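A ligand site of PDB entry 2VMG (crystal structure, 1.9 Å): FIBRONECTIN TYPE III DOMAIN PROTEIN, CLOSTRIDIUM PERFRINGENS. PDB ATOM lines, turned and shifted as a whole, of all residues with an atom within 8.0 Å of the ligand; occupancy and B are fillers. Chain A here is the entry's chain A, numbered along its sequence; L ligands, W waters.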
ATOM      1  N   GLY A  28     -10.980 -15.356  16.450  1.00  0.00           N
ATOM      2  CA  GLY A  28     -11.712 -15.407  15.189  1.00  0.00           C
ATOM      3  C   GLY A  28     -13.086 -16.060  15.214  1.00  0.00           C
ATOM      4  O   GLY A  28     -13.875 -15.864  14.285  1.00  0.00           O
ATOM      5  N   TYR A  29     -13.357 -16.820  16.265  1.00  0.00           N
ATOM      6  CA  TYR A  29     -14.587 -17.606  16.400  1.00  0.00           C
ATOM      7  C   TYR A  29     -14.785 -17.949  17.881  1.00  0.00           C
ATOM      8  O   TYR A  29     -13.874 -18.439  18.536  1.00  0.00           O
ATOM      9  CB  TYR A  29     -14.490 -18.876  15.565  1.00  0.00           C
ATOM     10  CG  TYR A  29     -15.673 -19.820  15.632  1.00  0.00           C
ATOM     11  CD1 TYR A  29     -16.764 -19.668  14.764  1.00  0.00           C
ATOM     12  CD2 TYR A  29     -15.700 -20.872  16.545  1.00  0.00           C
ATOM     13  CE1 TYR A  29     -17.846 -20.533  14.816  1.00  0.00           C
ATOM     14  CE2 TYR A  29     -16.781 -21.749  16.605  1.00  0.00           C
ATOM     15  CZ  TYR A  29     -17.855 -21.575  15.741  1.00  0.00           C
ATOM     16  OH  TYR A  29     -18.927 -22.439  15.793  1.00  0.00           O
ATOM     17  N   GLY A  30     -15.988 -17.696  18.384  1.00  0.00           N
ATOM     18  CA  GLY A  30     -16.316 -17.937  19.781  1.00  0.00           C
ATOM     19  C   GLY A  30     -15.627 -16.967  20.724  1.00  0.00           C
ATOM     20  O   GLY A  30     -15.477 -15.775  20.410  1.00  0.00           O
ATOM     21  N   CYS A  38     -11.138 -24.053  22.571  1.00  0.00           N
ATOM     22  CA  CYS A  38     -12.133 -23.157  21.995  1.00  0.00           C
ATOM     23  C   CYS A  38     -13.563 -23.618  22.295  1.00  0.00           C
ATOM     24  O   CYS A  38     -14.423 -22.816  22.661  1.00  0.00           O
ATOM     25  CB  CYS A  38     -11.922 -23.032  20.477  1.00  0.00           C
ATOM     26  SG  CYS A  38     -13.239 -22.149  19.592  1.00  0.00           S
ATOM     27  N   ASP A  39     -13.809 -24.921  22.146  1.00  0.00           N
ATOM     28  CA  ASP A  39     -15.136 -25.498  22.365  1.00  0.00           C
ATOM     29  C   ASP A  39     -15.382 -25.976  23.806  1.00  0.00           C
ATOM     30  O   ASP A  39     -16.332 -26.724  24.060  1.00  0.00           O
ATOM     31  CB  ASP A  39     -15.391 -26.638  21.359  1.00  0.00           C
ATOM     32  CG  ASP A  39     -15.534 -26.139  19.923  1.00  0.00           C
ATOM     33  OD1 ASP A  39     -15.607 -24.910  19.694  1.00  0.00           O
ATOM     34  OD2 ASP A  39     -15.595 -26.984  19.004  1.00  0.00           O
ATOM     35  N   HIS A  62      -8.759 -19.181  18.784  1.00  0.00           N
ATOM     36  CA  HIS A  62      -9.135 -19.468  17.398  1.00  0.00           C
ATOM     37  C   HIS A  62      -8.553 -18.400  16.472  1.00  0.00           C
ATOM     38  O   HIS A  62      -8.664 -17.196  16.743  1.00  0.00           O
ATOM     39  CB  HIS A  62     -10.667 -19.466  17.288  1.00  0.00           C
ATOM     40  CG  HIS A  62     -11.204 -20.187  16.091  1.00  0.00           C
ATOM     41  ND1 HIS A  62     -11.083 -19.687  14.809  1.00  0.00           N
ATOM     42  CD2 HIS A  62     -11.877 -21.357  15.981  1.00  0.00           C
ATOM     43  CE1 HIS A  62     -11.645 -20.526  13.959  1.00  0.00           C
ATOM     44  NE2 HIS A  62     -12.137 -21.551  14.642  1.00  0.00           N
ATOM     45  N   ALA A  63      -7.932 -18.832  15.365  1.00  0.00           N
ATOM     46  CA  ALA A  63      -7.452 -17.919  14.333  1.00  0.00           C
ATOM     47  C   ALA A  63      -8.628 -17.102  13.749  1.00  0.00           C
ATOM     48  O   ALA A  63      -9.712 -17.644  13.569  1.00  0.00           O
ATOM     49  CB  ALA A  63      -6.761 -18.697  13.225  1.00  0.00           C
ATOM     50  N   GLU A  89      -9.360 -31.589  19.583  1.00  0.00           N
ATOM     51  CA  GLU A  89     -10.795 -31.636  19.330  1.00  0.00           C
ATOM     52  C   GLU A  89     -11.055 -31.483  17.824  1.00  0.00           C
ATOM     53  O   GLU A  89     -12.082 -31.926  17.327  1.00  0.00           O
ATOM     54  CB  GLU A  89     -11.551 -30.555  20.131  1.00  0.00           C
ATOM     55  CG  GLU A  89     -11.416 -29.108  19.627  1.00  0.00           C
ATOM     56  CD  GLU A  89     -11.865 -28.079  20.658  1.00  0.00           C
ATOM     57  OE1 GLU A  89     -12.393 -28.474  21.723  1.00  0.00           O
ATOM     58  OE2 GLU A  89     -11.674 -26.859  20.419  1.00  0.00           O
ATOM     59  N   MET A  90     -10.095 -30.884  17.128  1.00  0.00           N
ATOM     60  CA  MET A  90     -10.178 -30.649  15.681  1.00  0.00           C
ATOM     61  C   MET A  90      -9.308 -31.596  14.851  1.00  0.00           C
ATOM     62  O   MET A  90      -9.002 -31.305  13.682  1.00  0.00           O
ATOM     63  CB  MET A  90      -9.862 -29.193  15.337  1.00  0.00           C
ATOM     64  CG  MET A  90     -10.821 -28.174  15.970  1.00  0.00           C
ATOM     65  SD  MET A  90     -12.575 -28.577  15.808  1.00  0.00           S
ATOM     66  CE  MET A  90     -12.786 -28.364  14.039  1.00  0.00           C
ATOM     67  N   THR A  93      -9.655 -32.677  10.730  1.00  0.00           N
ATOM     68  CA  THR A  93     -10.406 -31.611  10.066  1.00  0.00           C
ATOM     69  C   THR A  93      -9.485 -30.788   9.154  1.00  0.00           C
ATOM     70  O   THR A  93      -8.302 -31.128   9.003  1.00  0.00           O
ATOM     71  CB  THR A  93     -11.105 -30.658  11.065  1.00  0.00           C
ATOM     72  OG1 THR A  93     -10.120 -29.865  11.737  1.00  0.00           O
ATOM     73  CG2 THR A  93     -11.959 -31.432  12.077  1.00  0.00           C
ATOM     74  N   VAL A  94     -10.020 -29.709   8.572  1.00  0.00           N
ATOM     75  CA  VAL A  94      -9.233 -28.820   7.703  1.00  0.00           C
ATOM     76  C   VAL A  94      -8.364 -27.833   8.475  1.00  0.00           C
ATOM     77  O   VAL A  94      -7.768 -26.935   7.881  1.00  0.00           O
ATOM     78  CB  VAL A  94     -10.134 -28.031   6.694  1.00  0.00           C
ATOM     79  CG1 VAL A  94     -10.731 -28.964   5.648  1.00  0.00           C
ATOM     80  CG2 VAL A  94     -11.220 -27.227   7.424  1.00  0.00           C
ATOM     81  N   ALA A  95      -8.282 -28.002   9.799  1.00  0.00           N
ATOM     82  CA  ALA A  95      -7.506 -27.113  10.676  1.00  0.00           C
ATOM     83  C   ALA A  95      -6.084 -26.854  10.178  1.00  0.00           C
ATOM     84  O   ALA A  95      -5.315 -27.786   9.932  1.00  0.00           O
ATOM     85  CB  ALA A  95      -7.476 -27.668  12.099  1.00  0.00           C
ATOM     86  N   SER A 143      -8.452 -20.322   5.259  1.00  0.00           N
ATOM     87  CA  SER A 143      -9.587 -19.726   5.960  1.00  0.00           C
ATOM     88  C   SER A 143      -9.476 -20.092   7.432  1.00  0.00           C
ATOM     89  O   SER A 143      -8.630 -20.924   7.807  1.00  0.00           O
ATOM     90  CB  SER A 143     -10.925 -20.230   5.400  1.00  0.00           C
ATOM     91  OG  SER A 143     -11.204 -21.557   5.822  1.00  0.00           O
ATOM     92  N   ILE A 144     -10.316 -19.498   8.277  1.00  0.00           N
ATOM     93  CA  ILE A 144     -10.324 -19.796   9.712  1.00  0.00           C
ATOM     94  C   ILE A 144     -11.094 -21.070  10.079  1.00  0.00           C
ATOM     95  O   ILE A 144     -11.199 -21.422  11.250  1.00  0.00           O
ATOM     96  CB  ILE A 144     -10.827 -18.602  10.570  1.00  0.00           C
ATOM     97  CG1 ILE A 144     -12.337 -18.359  10.350  1.00  0.00           C
ATOM     98  CG2 ILE A 144      -9.982 -17.339  10.306  1.00  0.00           C
ATOM     99  CD1 ILE A 144     -13.028 -17.767  11.566  1.00  0.00           C
ATOM    100  N   GLY A 145     -11.626 -21.762   9.067  1.00  0.00           N
ATOM    101  CA  GLY A 145     -12.395 -22.977   9.289  1.00  0.00           C
ATOM    102  C   GLY A 145     -11.602 -24.029  10.058  1.00  0.00           C
ATOM    103  O   GLY A 145     -10.515 -24.421   9.623  1.00  0.00           O
ATOM    104  N   SER A 146     -12.140 -24.455  11.200  1.00  0.00           N
ATOM    105  CA  SER A 146     -11.529 -25.485  12.064  1.00  0.00           C
ATOM    106  C   SER A 146     -10.278 -25.028  12.826  1.00  0.00           C
ATOM    107  O   SER A 146      -9.638 -25.830  13.519  1.00  0.00           O
ATOM    108  CB  SER A 146     -11.220 -26.766  11.258  1.00  0.00           C
ATOM    109  OG  SER A 146     -12.399 -27.330  10.718  1.00  0.00           O
ATOM    110  N   ASP A 147      -9.943 -23.744  12.744  1.00  0.00           N
ATOM    111  CA  ASP A 147      -8.661 -23.239  13.231  1.00  0.00           C
ATOM    112  C   ASP A 147      -8.584 -23.046  14.753  1.00  0.00           C
ATOM    113  O   ASP A 147      -8.310 -21.940  15.220  1.00  0.00           O
ATOM    114  CB  ASP A 147      -8.298 -21.946  12.525  1.00  0.00           C
ATOM    115  CG  ASP A 147      -7.830 -22.158  11.086  1.00  0.00           C
ATOM    116  OD1 ASP A 147      -7.874 -23.307  10.593  1.00  0.00           O
ATOM    117  OD2 ASP A 147      -7.417 -21.172  10.455  1.00  0.00           O
ATOM    118  N   HIS A 148      -8.810 -24.120  15.503  1.00  0.00           N
ATOM    119  CA  HIS A 148      -8.708 -24.078  16.966  1.00  0.00           C
ATOM    120  C   HIS A 148      -7.245 -24.219  17.378  1.00  0.00           C
ATOM    121  O   HIS A 148      -6.633 -25.285  17.198  1.00  0.00           O
ATOM    122  CB  HIS A 148      -9.548 -25.191  17.602  1.00  0.00           C
ATOM    123  CG  HIS A 148     -11.009 -25.159  17.247  1.00  0.00           C
ATOM    124  ND1 HIS A 148     -11.983 -25.655  18.088  1.00  0.00           N
ATOM    125  CD2 HIS A 148     -11.663 -24.697  16.146  1.00  0.00           C
ATOM    126  CE1 HIS A 148     -13.173 -25.504  17.518  1.00  0.00           C
ATOM    127  NE2 HIS A 148     -13.001 -24.918  16.350  1.00  0.00           N
HETATM  128  C1  LIG L   1     -16.338 -24.646  11.408  1.00  0.00           C
HETATM  129  C2  LIG L   1     -15.843 -25.393  12.647  1.00  0.00           C
HETATM  130  C3  LIG L   1     -15.865 -24.464  13.865  1.00  0.00           C
HETATM  131  C4  LIG L   1     -15.070 -23.186  13.571  1.00  0.00           C
HETATM  132  C5  LIG L   1     -15.568 -22.535  12.280  1.00  0.00           C
HETATM  133  C6  LIG L   1     -14.742 -21.303  11.911  1.00  0.00           C
HETATM  134  C7  LIG L   1     -17.189 -25.157   9.255  1.00  0.00           C
HETATM  135  O1  LIG L   1     -16.250 -25.513  10.271  1.00  0.00           O
HETATM  136  O2  LIG L   1     -16.654 -26.549  12.915  1.00  0.00           O
HETATM  137  O3  LIG L   1     -15.341 -25.154  15.002  1.00  0.00           O
HETATM  138  O4  LIG L   1     -13.679 -23.509  13.462  1.00  0.00           O
HETATM  139  O5  LIG L   1     -15.543 -23.478  11.191  1.00  0.00           O
HETATM  140  O6  LIG L   1     -15.425 -20.552  10.907  1.00  0.00           O
HETATM  141  O   HOH W   1     -15.319 -21.136   8.384  1.00  0.00           O
HETATM  142  O   HOH W   2     -16.974 -18.391  11.205  1.00  0.00           O
HETATM  143  O   HOH W   3     -14.608 -28.599  11.574  1.00  0.00           O
HETATM  144  O   HOH W   4     -13.902 -25.816   8.775  1.00  0.00           O
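A ring nitrogen (NE2) of His 148 sits close to the side-chain sulfur (SD) of Met 90 (3.7 Å).
A ring nitrogen (ND1) of His 148 is in hydrogen-bond range of the side-chain carboxylate (OE2) of Glu 89 (2.6 Å).
N of Gly 28 lies within hydrogen-bond range of O of His 62, 3.0 Å away.
The backbone NH of Gly 145 sits close to the side-chain hydroxyl of Ser 143 (3.3 Å).
O of Asp 147 sits at hydrogen-bond distance from N of Ala 63 (3.1 Å).
A ring nitrogen (NE2) of His 148 lies within hydrogen-bond range of an oxygen (O3) of the ligand (2.7 Å).
A ring nitrogen (NE2) of His 62 sits at hydrogen-bond distance from an oxygen (O4) of the ligand (2.8 Å).
O4 of the ligand is in hydrogen-bond range of N of Ser 146 (2.9 Å).
Water W4 bridges an oxygen (O1) of the ligand and the side-chain hydroxyl (OG) of Ser 146.
Water W3 bridges the side-chain hydroxyl (OG) of Ser 146 (2.7 Å) and an oxygen (O2) of the ligand (3.2 Å).
Merely in contact with the ligand: Ile 144, Gly 145, Tyr 29 and Asp 147.
Of the 18 residues printed, 7 come within 4 Å of the ligand.
The nearest printed residue that does not touch the ligand is Met 90 (4.2 Å).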
